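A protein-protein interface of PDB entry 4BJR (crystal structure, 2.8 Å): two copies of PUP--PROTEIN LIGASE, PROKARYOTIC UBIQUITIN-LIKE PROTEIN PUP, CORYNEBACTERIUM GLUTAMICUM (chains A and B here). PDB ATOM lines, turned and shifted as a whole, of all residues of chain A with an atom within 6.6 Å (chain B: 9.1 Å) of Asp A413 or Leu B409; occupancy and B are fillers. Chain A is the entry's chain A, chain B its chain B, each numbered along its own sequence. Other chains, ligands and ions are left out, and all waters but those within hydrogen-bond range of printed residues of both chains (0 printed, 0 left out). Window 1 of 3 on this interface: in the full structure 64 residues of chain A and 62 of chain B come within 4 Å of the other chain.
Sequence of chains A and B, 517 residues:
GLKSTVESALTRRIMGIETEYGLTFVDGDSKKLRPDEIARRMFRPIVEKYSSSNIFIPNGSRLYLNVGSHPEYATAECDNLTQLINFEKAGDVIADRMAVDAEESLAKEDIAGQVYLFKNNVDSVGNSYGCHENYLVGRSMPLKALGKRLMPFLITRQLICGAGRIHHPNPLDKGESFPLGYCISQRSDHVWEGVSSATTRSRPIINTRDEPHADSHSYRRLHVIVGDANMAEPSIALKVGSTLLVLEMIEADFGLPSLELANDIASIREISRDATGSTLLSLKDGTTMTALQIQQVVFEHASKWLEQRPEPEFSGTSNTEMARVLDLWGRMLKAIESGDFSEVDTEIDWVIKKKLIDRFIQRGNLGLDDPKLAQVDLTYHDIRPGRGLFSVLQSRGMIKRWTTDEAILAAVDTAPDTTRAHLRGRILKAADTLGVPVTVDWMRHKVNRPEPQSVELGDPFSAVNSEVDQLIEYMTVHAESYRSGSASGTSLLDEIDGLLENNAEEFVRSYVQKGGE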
ATOM      1  N   PRO A  58      -2.844 -17.429 -16.733  1.00  0.00           N
ATOM      2  CA  PRO A  58      -3.302 -16.221 -16.050  1.00  0.00           C
ATOM      3  C   PRO A  58      -3.028 -14.904 -16.758  1.00  0.00           C
ATOM      4  O   PRO A  58      -3.744 -13.955 -16.501  1.00  0.00           O
ATOM      5  CB  PRO A  58      -2.548 -16.282 -14.733  1.00  0.00           C
ATOM      6  CG  PRO A  58      -2.437 -17.687 -14.473  1.00  0.00           C
ATOM      7  CD  PRO A  58      -2.160 -18.321 -15.788  1.00  0.00           C
ATOM      8  N   ASN A  59      -1.980 -14.810 -17.560  1.00  0.00           N
ATOM      9  CA  ASN A  59      -1.761 -13.593 -18.325  1.00  0.00           C
ATOM     10  C   ASN A  59      -2.800 -13.397 -19.426  1.00  0.00           C
ATOM     11  O   ASN A  59      -2.862 -12.351 -20.042  1.00  0.00           O
ATOM     12  CB  ASN A  59      -0.338 -13.537 -18.893  1.00  0.00           C
ATOM     13  CG  ASN A  59      -0.135 -14.384 -20.123  1.00  0.00           C
ATOM     14  OD1 ASN A  59      -1.009 -15.115 -20.557  1.00  0.00           O
ATOM     15  ND2 ASN A  59       1.034 -14.253 -20.715  1.00  0.00           N
ATOM     16  N   GLY A  60      -3.551 -14.442 -19.733  1.00  0.00           N
ATOM     17  CA  GLY A  60      -4.678 -14.332 -20.642  1.00  0.00           C
ATOM     18  C   GLY A  60      -4.399 -14.902 -22.011  1.00  0.00           C
ATOM     19  O   GLY A  60      -5.266 -14.962 -22.868  1.00  0.00           O
ATOM     20  N   ALA A  90       7.100 -12.790 -23.794  1.00  0.00           N
ATOM     21  CA  ALA A  90       6.709 -13.495 -22.590  1.00  0.00           C
ATOM     22  C   ALA A  90       6.474 -14.958 -22.897  1.00  0.00           C
ATOM     23  O   ALA A  90       6.791 -15.843 -22.094  1.00  0.00           O
ATOM     24  CB  ALA A  90       5.478 -12.876 -22.005  1.00  0.00           C
ATOM     25  N   ILE A  94       7.998 -18.347 -20.984  1.00  0.00           N
ATOM     26  CA  ILE A  94       7.222 -19.453 -20.449  1.00  0.00           C
ATOM     27  C   ILE A  94       7.606 -20.777 -21.082  1.00  0.00           C
ATOM     28  O   ILE A  94       7.829 -21.781 -20.395  1.00  0.00           O
ATOM     29  CB  ILE A  94       5.735 -19.227 -20.670  1.00  0.00           C
ATOM     30  CG1 ILE A  94       5.282 -17.989 -19.919  1.00  0.00           C
ATOM     31  CG2 ILE A  94       4.955 -20.426 -20.227  1.00  0.00           C
ATOM     32  CD1 ILE A  94       4.081 -17.335 -20.513  1.00  0.00           C
ATOM     33  N   ARG A  97      10.843 -22.093 -19.899  1.00  0.00           N
ATOM     34  CA  ARG A  97      10.746 -22.673 -18.571  1.00  0.00           C
ATOM     35  C   ARG A  97      10.237 -24.100 -18.662  1.00  0.00           C
ATOM     36  O   ARG A  97      10.767 -25.014 -18.023  1.00  0.00           O
ATOM     37  CB  ARG A  97       9.829 -21.847 -17.684  1.00  0.00           C
ATOM     38  CG  ARG A  97      10.342 -20.460 -17.418  1.00  0.00           C
ATOM     39  CD  ARG A  97       9.783 -19.884 -16.148  1.00  0.00           C
ATOM     40  NE  ARG A  97      10.150 -18.485 -15.985  1.00  0.00           N
ATOM     41  CZ  ARG A  97       9.325 -17.555 -15.529  1.00  0.00           C
ATOM     42  NH1 ARG A  97       8.098 -17.886 -15.174  1.00  0.00           N
ATOM     43  NH2 ARG A  97       9.728 -16.303 -15.420  1.00  0.00           N
ATOM     44  N   ILE A 408       8.642  -7.324 -20.106  1.00  0.00           N
ATOM     45  CA  ILE A 408       8.408  -8.686 -20.552  1.00  0.00           C
ATOM     46  C   ILE A 408       8.135  -9.590 -19.362  1.00  0.00           C
ATOM     47  O   ILE A 408       7.193 -10.384 -19.355  1.00  0.00           O
ATOM     48  CB  ILE A 408       9.612  -9.207 -21.332  1.00  0.00           C
ATOM     49  CG1 ILE A 408       9.835  -8.357 -22.575  1.00  0.00           C
ATOM     50  CG2 ILE A 408       9.432 -10.650 -21.687  1.00  0.00           C
ATOM     51  CD1 ILE A 408      11.134  -8.607 -23.257  1.00  0.00           C
ATOM     52  N   LEU A 409       8.960  -9.442 -18.339  1.00  0.00           N
ATOM     53  CA  LEU A 409       8.816 -10.236 -17.138  1.00  0.00           C
ATOM     54  C   LEU A 409       7.471  -9.982 -16.487  1.00  0.00           C
ATOM     55  O   LEU A 409       6.861 -10.880 -15.931  1.00  0.00           O
ATOM     56  CB  LEU A 409       9.942  -9.933 -16.163  1.00  0.00           C
ATOM     57  CG  LEU A 409      11.152 -10.833 -16.313  1.00  0.00           C
ATOM     58  CD1 LEU A 409      12.363 -10.185 -15.709  1.00  0.00           C
ATOM     59  CD2 LEU A 409      10.869 -12.136 -15.633  1.00  0.00           C
ATOM     60  N   ALA A 410       7.021  -8.739 -16.538  1.00  0.00           N
ATOM     61  CA  ALA A 410       5.699  -8.407 -16.048  1.00  0.00           C
ATOM     62  C   ALA A 410       4.640  -9.076 -16.905  1.00  0.00           C
ATOM     63  O   ALA A 410       3.624  -9.535 -16.405  1.00  0.00           O
ATOM     64  CB  ALA A 410       5.503  -6.920 -16.033  1.00  0.00           C
ATOM     65  N   ALA A 411       4.886  -9.104 -18.205  1.00  0.00           N
ATOM     66  CA  ALA A 411       3.953  -9.683 -19.157  1.00  0.00           C
ATOM     67  C   ALA A 411       3.733 -11.173 -18.949  1.00  0.00           C
ATOM     68  O   ALA A 411       2.658 -11.676 -19.239  1.00  0.00           O
ATOM     69  CB  ALA A 411       4.418  -9.422 -20.561  1.00  0.00           C
ATOM     70  N   VAL A 412       4.751 -11.900 -18.509  1.00  0.00           N
ATOM     71  CA  VAL A 412       4.545 -13.328 -18.286  1.00  0.00           C
ATOM     72  C   VAL A 412       3.511 -13.588 -17.185  1.00  0.00           C
ATOM     73  O   VAL A 412       2.708 -14.505 -17.290  1.00  0.00           O
ATOM     74  CB  VAL A 412       5.864 -14.082 -17.963  1.00  0.00           C
ATOM     75  CG1 VAL A 412       6.953 -13.695 -18.929  1.00  0.00           C
ATOM     76  CG2 VAL A 412       6.328 -13.848 -16.554  1.00  0.00           C
ATOM     77  N   ASP A 413       3.567 -12.805 -16.114  1.00  0.00           N
ATOM     78  CA  ASP A 413       2.673 -12.952 -14.970  1.00  0.00           C
ATOM     79  C   ASP A 413       1.270 -12.364 -15.118  1.00  0.00           C
ATOM     80  O   ASP A 413       0.303 -12.978 -14.695  1.00  0.00           O
ATOM     81  CB  ASP A 413       3.342 -12.349 -13.742  1.00  0.00           C
ATOM     82  CG  ASP A 413       4.373 -13.274 -13.137  1.00  0.00           C
ATOM     83  OD1 ASP A 413       4.255 -14.503 -13.311  1.00  0.00           O
ATOM     84  OD2 ASP A 413       5.317 -12.767 -12.508  1.00  0.00           O
ATOM     85  N   THR A 414       1.161 -11.174 -15.696  1.00  0.00           N
ATOM     86  CA  THR A 414      -0.101 -10.452 -15.666  1.00  0.00           C
ATOM     87  C   THR A 414      -0.647 -10.066 -17.022  1.00  0.00           C
ATOM     88  O   THR A 414       0.088  -9.772 -17.954  1.00  0.00           O
ATOM     89  CB  THR A 414       0.015  -9.155 -14.872  1.00  0.00           C
ATOM     90  OG1 THR A 414       0.914  -8.271 -15.545  1.00  0.00           O
ATOM     91  CG2 THR A 414       0.535  -9.427 -13.515  1.00  0.00           C
ATOM     92  N   ALA A 415      -1.967 -10.038 -17.094  1.00  0.00           N
ATOM     93  CA  ALA A 415      -2.679  -9.770 -18.323  1.00  0.00           C
ATOM     94  C   ALA A 415      -2.604  -8.308 -18.695  1.00  0.00           C
ATOM     95  O   ALA A 415      -2.342  -7.471 -17.844  1.00  0.00           O
ATOM     96  CB  ALA A 415      -4.113 -10.206 -18.186  1.00  0.00           C
ATOM     97  N   LYS A 429      -6.764 -16.018 -12.186  1.00  0.00           N
ATOM     98  CA  LYS A 429      -5.955 -15.905 -10.991  1.00  0.00           C
ATOM     99  C   LYS A 429      -6.792 -16.290  -9.807  1.00  0.00           C
ATOM    100  O   LYS A 429      -6.389 -17.124  -8.997  1.00  0.00           O
ATOM    101  CB  LYS A 429      -5.398 -14.499 -10.828  1.00  0.00           C
ATOM    102  CG  LYS A 429      -4.534 -14.052 -11.968  1.00  0.00           C
ATOM    103  CD  LYS A 429      -3.212 -13.540 -11.466  1.00  0.00           C
ATOM    104  CE  LYS A 429      -2.535 -12.690 -12.508  1.00  0.00           C
ATOM    105  NZ  LYS A 429      -1.945 -11.460 -11.945  1.00  0.00           N
ATOM    106  N   ASN B  59      16.845  -2.592  -8.245  1.00  0.00           N
ATOM    107  CA  ASN B  59      15.613  -2.009  -7.737  1.00  0.00           C
ATOM    108  C   ASN B  59      15.880  -0.799  -6.854  1.00  0.00           C
ATOM    109  O   ASN B  59      14.973  -0.064  -6.520  1.00  0.00           O
ATOM    110  CB  ASN B  59      14.755  -3.056  -7.022  1.00  0.00           C
ATOM    111  CG  ASN B  59      15.255  -3.415  -5.655  1.00  0.00           C
ATOM    112  OD1 ASN B  59      16.314  -2.988  -5.228  1.00  0.00           O
ATOM    113  ND2 ASN B  59      14.475  -4.205  -4.949  1.00  0.00           N
ATOM    114  N   ILE B  85       5.556  -1.693   1.172  1.00  0.00           N
ATOM    115  CA  ILE B  85       5.294  -3.084   1.466  1.00  0.00           C
ATOM    116  C   ILE B  85       5.790  -3.950   0.333  1.00  0.00           C
ATOM    117  O   ILE B  85       6.413  -4.979   0.557  1.00  0.00           O
ATOM    118  CB  ILE B  85       3.815  -3.343   1.683  1.00  0.00           C
ATOM    119  CG1 ILE B  85       3.342  -2.624   2.932  1.00  0.00           C
ATOM    120  CG2 ILE B  85       3.560  -4.810   1.840  1.00  0.00           C
ATOM    121  CD1 ILE B  85       1.886  -2.777   3.187  1.00  0.00           C
ATOM    122  N   ASN B  86       5.544  -3.507  -0.889  1.00  0.00           N
ATOM    123  CA  ASN B  86       5.951  -4.276  -2.050  1.00  0.00           C
ATOM    124  C   ASN B  86       7.436  -4.531  -2.084  1.00  0.00           C
ATOM    125  O   ASN B  86       7.869  -5.654  -2.279  1.00  0.00           O
ATOM    126  CB  ASN B  86       5.546  -3.568  -3.336  1.00  0.00           C
ATOM    127  CG  ASN B  86       4.070  -3.597  -3.578  1.00  0.00           C
ATOM    128  OD1 ASN B  86       3.392  -4.554  -3.234  1.00  0.00           O
ATOM    129  ND2 ASN B  86       3.563  -2.559  -4.209  1.00  0.00           N
ATOM    130  N   PHE B  87       8.221  -3.485  -1.878  1.00  0.00           N
ATOM    131  CA  PHE B  87       9.669  -3.645  -1.930  1.00  0.00           C
ATOM    132  C   PHE B  87      10.217  -4.421  -0.741  1.00  0.00           C
ATOM    133  O   PHE B  87      11.168  -5.204  -0.868  1.00  0.00           O
ATOM    134  CB  PHE B  87      10.328  -2.279  -2.070  1.00  0.00           C
ATOM    135  CG  PHE B  87      10.257  -1.750  -3.459  1.00  0.00           C
ATOM    136  CD1 PHE B  87       9.120  -1.127  -3.915  1.00  0.00           C
ATOM    137  CD2 PHE B  87      11.299  -1.930  -4.328  1.00  0.00           C
ATOM    138  CE1 PHE B  87       9.045  -0.677  -5.194  1.00  0.00           C
ATOM    139  CE2 PHE B  87      11.224  -1.476  -5.606  1.00  0.00           C
ATOM    140  CZ  PHE B  87      10.096  -0.857  -6.040  1.00  0.00           C
ATOM    141  N   LYS B  89       8.654  -6.820   0.750  1.00  0.00           N
ATOM    142  CA  LYS B  89       8.356  -8.190   0.404  1.00  0.00           C
ATOM    143  C   LYS B  89       9.288  -8.708  -0.674  1.00  0.00           C
ATOM    144  O   LYS B  89       9.649  -9.876  -0.679  1.00  0.00           O
ATOM    145  CB  LYS B  89       6.907  -8.305  -0.040  1.00  0.00           C
ATOM    146  CG  LYS B  89       5.930  -8.340   1.105  1.00  0.00           C
ATOM    147  CD  LYS B  89       6.393  -9.287   2.180  1.00  0.00           C
ATOM    148  CE  LYS B  89       5.232  -9.816   2.970  1.00  0.00           C
ATOM    149  NZ  LYS B  89       5.692 -10.504   4.193  1.00  0.00           N
ATOM    150  N   ALA B  90       9.661  -7.830  -1.593  1.00  0.00           N
ATOM    151  CA  ALA B  90      10.587  -8.174  -2.660  1.00  0.00           C
ATOM    152  C   ALA B  90      11.917  -8.637  -2.096  1.00  0.00           C
ATOM    153  O   ALA B  90      12.589  -9.520  -2.648  1.00  0.00           O
ATOM    154  CB  ALA B  90      10.788  -6.992  -3.567  1.00  0.00           C
ATOM    155  N   GLY B  91      12.292  -8.036  -0.979  1.00  0.00           N
ATOM    156  CA  GLY B  91      13.523  -8.418  -0.322  1.00  0.00           C
ATOM    157  C   GLY B  91      13.556  -9.877   0.071  1.00  0.00           C
ATOM    158  O   GLY B  91      14.598 -10.523   0.009  1.00  0.00           O
ATOM    159  N   ASP B  92      12.408 -10.393   0.480  1.00  0.00           N
ATOM    160  CA  ASP B  92      12.297 -11.790   0.837  1.00  0.00           C
ATOM    161  C   ASP B  92      12.580 -12.680  -0.350  1.00  0.00           C
ATOM    162  O   ASP B  92      13.251 -13.696  -0.226  1.00  0.00           O
ATOM    163  CB  ASP B  92      10.912 -12.100   1.388  1.00  0.00           C
ATOM    164  CG  ASP B  92      10.714 -11.569   2.777  1.00  0.00           C
ATOM    165  OD1 ASP B  92      11.685 -11.040   3.343  1.00  0.00           O
ATOM    166  OD2 ASP B  92       9.595 -11.692   3.308  1.00  0.00           O
ATOM    167  N   VAL B  93      12.052 -12.303  -1.500  1.00  0.00           N
ATOM    168  CA  VAL B  93      12.266 -13.077  -2.699  1.00  0.00           C
ATOM    169  C   VAL B  93      13.729 -13.109  -3.050  1.00  0.00           C
ATOM    170  O   VAL B  93      14.301 -14.170  -3.263  1.00  0.00           O
ATOM    171  CB  VAL B  93      11.475 -12.508  -3.865  1.00  0.00           C
ATOM    172  CG1 VAL B  93      11.839 -13.212  -5.134  1.00  0.00           C
ATOM    173  CG2 VAL B  93      10.010 -12.639  -3.593  1.00  0.00           C
ATOM    174  N   ILE B  94      14.355 -11.947  -3.040  1.00  0.00           N
ATOM    175  CA  ILE B  94      15.750 -11.888  -3.424  1.00  0.00           C
ATOM    176  C   ILE B  94      16.617 -12.710  -2.488  1.00  0.00           C
ATOM    177  O   ILE B  94      17.450 -13.521  -2.915  1.00  0.00           O
ATOM    178  CB  ILE B  94      16.241 -10.453  -3.435  1.00  0.00           C
ATOM    179  CG1 ILE B  94      15.510  -9.669  -4.512  1.00  0.00           C
ATOM    180  CG2 ILE B  94      17.712 -10.408  -3.693  1.00  0.00           C
ATOM    181  CD1 ILE B  94      15.440  -8.210  -4.244  1.00  0.00           C
ATOM    182  N   ARG B  97      16.199 -16.406  -2.865  1.00  0.00           N
ATOM    183  CA  ARG B  97      16.872 -16.866  -4.064  1.00  0.00           C
ATOM    184  C   ARG B  97      18.332 -17.102  -3.781  1.00  0.00           C
ATOM    185  O   ARG B  97      18.901 -18.132  -4.152  1.00  0.00           O
ATOM    186  CB  ARG B  97      16.731 -15.854  -5.188  1.00  0.00           C
ATOM    187  CG  ARG B  97      15.326 -15.678  -5.690  1.00  0.00           C
ATOM    188  CD  ARG B  97      15.318 -15.152  -7.103  1.00  0.00           C
ATOM    189  NE  ARG B  97      13.974 -14.870  -7.583  1.00  0.00           N
ATOM    190  CZ  ARG B  97      13.650 -13.830  -8.336  1.00  0.00           C
ATOM    191  NH1 ARG B  97      14.576 -12.969  -8.716  1.00  0.00           N
ATOM    192  NH2 ARG B  97      12.399 -13.670  -8.728  1.00  0.00           N
ATOM    193  N   ARG B 401      -4.357 -10.118   2.516  1.00  0.00           N
ATOM    194  CA  ARG B 401      -3.353  -9.481   1.673  1.00  0.00           C
ATOM    195  C   ARG B 401      -3.615  -7.997   1.498  1.00  0.00           C
ATOM    196  O   ARG B 401      -4.717  -7.596   1.162  1.00  0.00           O
ATOM    197  CB  ARG B 401      -3.292 -10.141   0.303  1.00  0.00           C
ATOM    198  CG  ARG B 401      -3.104 -11.622   0.337  1.00  0.00           C
ATOM    199  CD  ARG B 401      -1.685 -11.976   0.646  1.00  0.00           C
ATOM    200  NE  ARG B 401      -0.737 -11.089  -0.002  1.00  0.00           N
ATOM    201  CZ  ARG B 401      -0.168 -11.349  -1.166  1.00  0.00           C
ATOM    202  NH1 ARG B 401      -0.461 -12.462  -1.807  1.00  0.00           N
ATOM    203  NH2 ARG B 401       0.696 -10.500  -1.685  1.00  0.00           N
ATOM    204  N   THR B 403      -1.423  -6.290  -0.578  1.00  0.00           N
ATOM    205  CA  THR B 403      -0.958  -6.059  -1.932  1.00  0.00           C
ATOM    206  C   THR B 403      -0.882  -7.340  -2.744  1.00  0.00           C
ATOM    207  O   THR B 403      -0.852  -8.426  -2.197  1.00  0.00           O
ATOM    208  CB  THR B 403       0.418  -5.397  -1.932  1.00  0.00           C
ATOM    209  OG1 THR B 403       0.832  -5.150  -3.276  1.00  0.00           O
ATOM    210  CG2 THR B 403       1.425  -6.294  -1.272  1.00  0.00           C
ATOM    211  N   THR B 404      -0.880  -7.204  -4.059  1.00  0.00           N
ATOM    212  CA  THR B 404      -0.809  -8.353  -4.941  1.00  0.00           C
ATOM    213  C   THR B 404       0.583  -8.936  -5.003  1.00  0.00           C
ATOM    214  O   THR B 404       1.562  -8.269  -4.727  1.00  0.00           O
ATOM    215  CB  THR B 404      -1.242  -8.006  -6.355  1.00  0.00           C
ATOM    216  OG1 THR B 404      -0.128  -7.482  -7.080  1.00  0.00           O
ATOM    217  CG2 THR B 404      -2.345  -6.988  -6.319  1.00  0.00           C
ATOM    218  N   ASP B 405       0.650 -10.202  -5.370  1.00  0.00           N
ATOM    219  CA  ASP B 405       1.902 -10.908  -5.521  1.00  0.00           C
ATOM    220  C   ASP B 405       2.726 -10.314  -6.644  1.00  0.00           C
ATOM    221  O   ASP B 405       3.946 -10.168  -6.563  1.00  0.00           O
ATOM    222  CB  ASP B 405       1.616 -12.374  -5.813  1.00  0.00           C
ATOM    223  CG  ASP B 405       1.665 -13.231  -4.584  1.00  0.00           C
ATOM    224  OD1 ASP B 405       2.092 -12.741  -3.525  1.00  0.00           O
ATOM    225  OD2 ASP B 405       1.262 -14.401  -4.673  1.00  0.00           O
ATOM    226  N   GLU B 406       2.019  -9.993  -7.711  1.00  0.00           N
ATOM    227  CA  GLU B 406       2.610  -9.535  -8.949  1.00  0.00           C
ATOM    228  C   GLU B 406       3.330  -8.212  -8.787  1.00  0.00           C
ATOM    229  O   GLU B 406       4.339  -7.969  -9.430  1.00  0.00           O
ATOM    230  CB  GLU B 406       1.533  -9.405 -10.013  1.00  0.00           C
ATOM    231  CG  GLU B 406       0.856 -10.717 -10.371  1.00  0.00           C
ATOM    232  CD  GLU B 406      -0.133 -11.183  -9.318  1.00  0.00           C
ATOM    233  OE1 GLU B 406      -0.969 -10.365  -8.880  1.00  0.00           O
ATOM    234  OE2 GLU B 406      -0.082 -12.366  -8.934  1.00  0.00           O
ATOM    235  N   ALA B 407       2.784  -7.344  -7.947  1.00  0.00           N
ATOM    236  CA  ALA B 407       3.418  -6.068  -7.654  1.00  0.00           C
ATOM    237  C   ALA B 407       4.750  -6.279  -6.969  1.00  0.00           C
ATOM    238  O   ALA B 407       5.710  -5.571  -7.227  1.00  0.00           O
ATOM    239  CB  ALA B 407       2.517  -5.220  -6.801  1.00  0.00           C
ATOM    240  N   ILE B 408       4.791  -7.260  -6.084  1.00  0.00           N
ATOM    241  CA  ILE B 408       6.012  -7.626  -5.401  1.00  0.00           C
ATOM    242  C   ILE B 408       7.027  -8.115  -6.400  1.00  0.00           C
ATOM    243  O   ILE B 408       8.188  -7.711  -6.389  1.00  0.00           O
ATOM    244  CB  ILE B 408       5.762  -8.731  -4.373  1.00  0.00           C
ATOM    245  CG1 ILE B 408       4.838  -8.236  -3.275  1.00  0.00           C
ATOM    246  CG2 ILE B 408       7.056  -9.213  -3.779  1.00  0.00           C
ATOM    247  CD1 ILE B 408       4.345  -9.322  -2.390  1.00  0.00           C
ATOM    248  N   LEU B 409       6.565  -8.981  -7.284  1.00  0.00           N
ATOM    249  CA  LEU B 409       7.441  -9.562  -8.275  1.00  0.00           C
ATOM    250  C   LEU B 409       8.008  -8.496  -9.179  1.00  0.00           C
ATOM    251  O   LEU B 409       9.152  -8.572  -9.593  1.00  0.00           O
ATOM    252  CB  LEU B 409       6.704 -10.618  -9.082  1.00  0.00           C
ATOM    253  CG  LEU B 409       7.446 -11.948  -9.152  1.00  0.00           C
ATOM    254  CD1 LEU B 409       7.964 -12.320  -7.785  1.00  0.00           C
ATOM    255  CD2 LEU B 409       6.538 -13.024  -9.657  1.00  0.00           C
ATOM    256  N   ALA B 410       7.198  -7.503  -9.498  1.00  0.00           N
ATOM    257  CA  ALA B 410       7.679  -6.376 -10.271  1.00  0.00           C
ATOM    258  C   ALA B 410       8.702  -5.599  -9.471  1.00  0.00           C
ATOM    259  O   ALA B 410       9.702  -5.161 -10.003  1.00  0.00           O
ATOM    260  CB  ALA B 410       6.538  -5.491 -10.671  1.00  0.00           C
ATOM    261  N   ALA B 411       8.445  -5.453  -8.182  1.00  0.00           N
ATOM    262  CA  ALA B 411       9.318  -4.703  -7.300  1.00  0.00           C
ATOM    263  C   ALA B 411      10.703  -5.311  -7.207  1.00  0.00           C
ATOM    264  O   ALA B 411      11.670  -4.600  -7.002  1.00  0.00           O
ATOM    265  CB  ALA B 411       8.712  -4.596  -5.939  1.00  0.00           C
ATOM    266  N   VAL B 412      10.802  -6.627  -7.321  1.00  0.00           N
ATOM    267  CA  VAL B 412      12.107  -7.273  -7.250  1.00  0.00           C
ATOM    268  C   VAL B 412      13.034  -6.777  -8.352  1.00  0.00           C
ATOM    269  O   VAL B 412      14.214  -6.526  -8.126  1.00  0.00           O
ATOM    270  CB  VAL B 412      11.988  -8.805  -7.368  1.00  0.00           C
ATOM    271  CG1 VAL B 412      13.333  -9.428  -7.611  1.00  0.00           C
ATOM    272  CG2 VAL B 412      11.391  -9.394  -6.128  1.00  0.00           C
ATOM    273  N   ASP B 413      12.488  -6.663  -9.552  1.00  0.00           N
ATOM    274  CA  ASP B 413      13.234  -6.237 -10.727  1.00  0.00           C
ATOM    275  C   ASP B 413      13.485  -4.739 -10.885  1.00  0.00           C
ATOM    276  O   ASP B 413      14.583  -4.333 -11.233  1.00  0.00           O
ATOM    277  CB  ASP B 413      12.509  -6.751 -11.962  1.00  0.00           C
ATOM    278  CG  ASP B 413      12.773  -8.215 -12.221  1.00  0.00           C
ATOM    279  OD1 ASP B 413      13.840  -8.714 -11.806  1.00  0.00           O
ATOM    280  OD2 ASP B 413      11.894  -8.875 -12.804  1.00  0.00           O
ATOM    281  N   THR B 414      12.465  -3.923 -10.648  1.00  0.00           N
ATOM    282  CA  THR B 414      12.546  -2.515 -11.003  1.00  0.00           C
ATOM    283  C   THR B 414      12.236  -1.568  -9.852  1.00  0.00           C
ATOM    284  O   THR B 414      11.432  -1.862  -8.979  1.00  0.00           O
ATOM    285  CB  THR B 414      11.612  -2.193 -12.186  1.00  0.00           C
ATOM    286  OG1 THR B 414      11.436  -0.779 -12.298  1.00  0.00           O
ATOM    287  CG2 THR B 414      10.278  -2.817 -11.988  1.00  0.00           C
ATOM    288  N   ALA B 415      12.881  -0.411  -9.899  1.00  0.00           N
ATOM    289  CA  ALA B 415      12.839   0.600  -8.852  1.00  0.00           C
ATOM    290  C   ALA B 415      11.530   1.362  -8.765  1.00  0.00           C
ATOM    291  O   ALA B 415      10.763   1.379  -9.713  1.00  0.00           O
ATOM    292  CB  ALA B 415      13.974   1.568  -9.063  1.00  0.00           C
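The side-chain carboxylate (OE1) of Glu B406 lies within salt-bridge range of the side-chain amino group (NZ) of Lys A429 (3.4 Å).
The side-chain hydroxyl (OG1) of Thr B404 lies close to the backbone NH (N) of Glu B406 (3.4 Å).
The side-chain hydroxyl of Thr A414 sits at hydrogen-bond distance from the backbone carbonyl oxygen of Ala A410 (3.1 Å).
Among the printed residues, merely in contact across the chains: Asp A413 with Leu B409, Leu A409 with Asp B413 and Thr A414 with Glu B406.
Printed residues of chain B within 4 Å of Leu A409: Asp B413 (3.2 Å).
No residue of chain B comes within 4 Å of Val A412.
Asp A413 touches just one residue of chain B: Leu B409.
Printed residues of chain B within 4 Å of Lys A429: Glu B406.
Ile B85 touches none of the printed residues of chain A.
Ala B90 touches none of the printed residues of chain A.
Of the printed residues of chain A, Glu B406 touches Thr A414 (3.4 Å) and Lys A429 (3.2 Å).
Of the printed residues of chain A, Leu B409 touches Asp A413.
Printed residues of chain A within 4 Å of Asp B413: Leu A409 (3.2 Å).
The nearest printed residue of chain A that does not touch Asp B413 is Ala A410 (6.1 Å).
Of the 15 printed residues of chain A, 4 touch a printed residue of chain B.
Among the printed residues, Asp or Glu carboxylates within 4 Å of a Lys or Arg side-chain nitrogen of the other chain: Lys A429 with Glu B406.
Leu A409 touches Asp B413, and with the chains exchanged Asp A413 touches Leu B409.
Of the 4 pairs that touch across the chains among the printed residues, 2 have their exchanged pair printed and touching as well.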
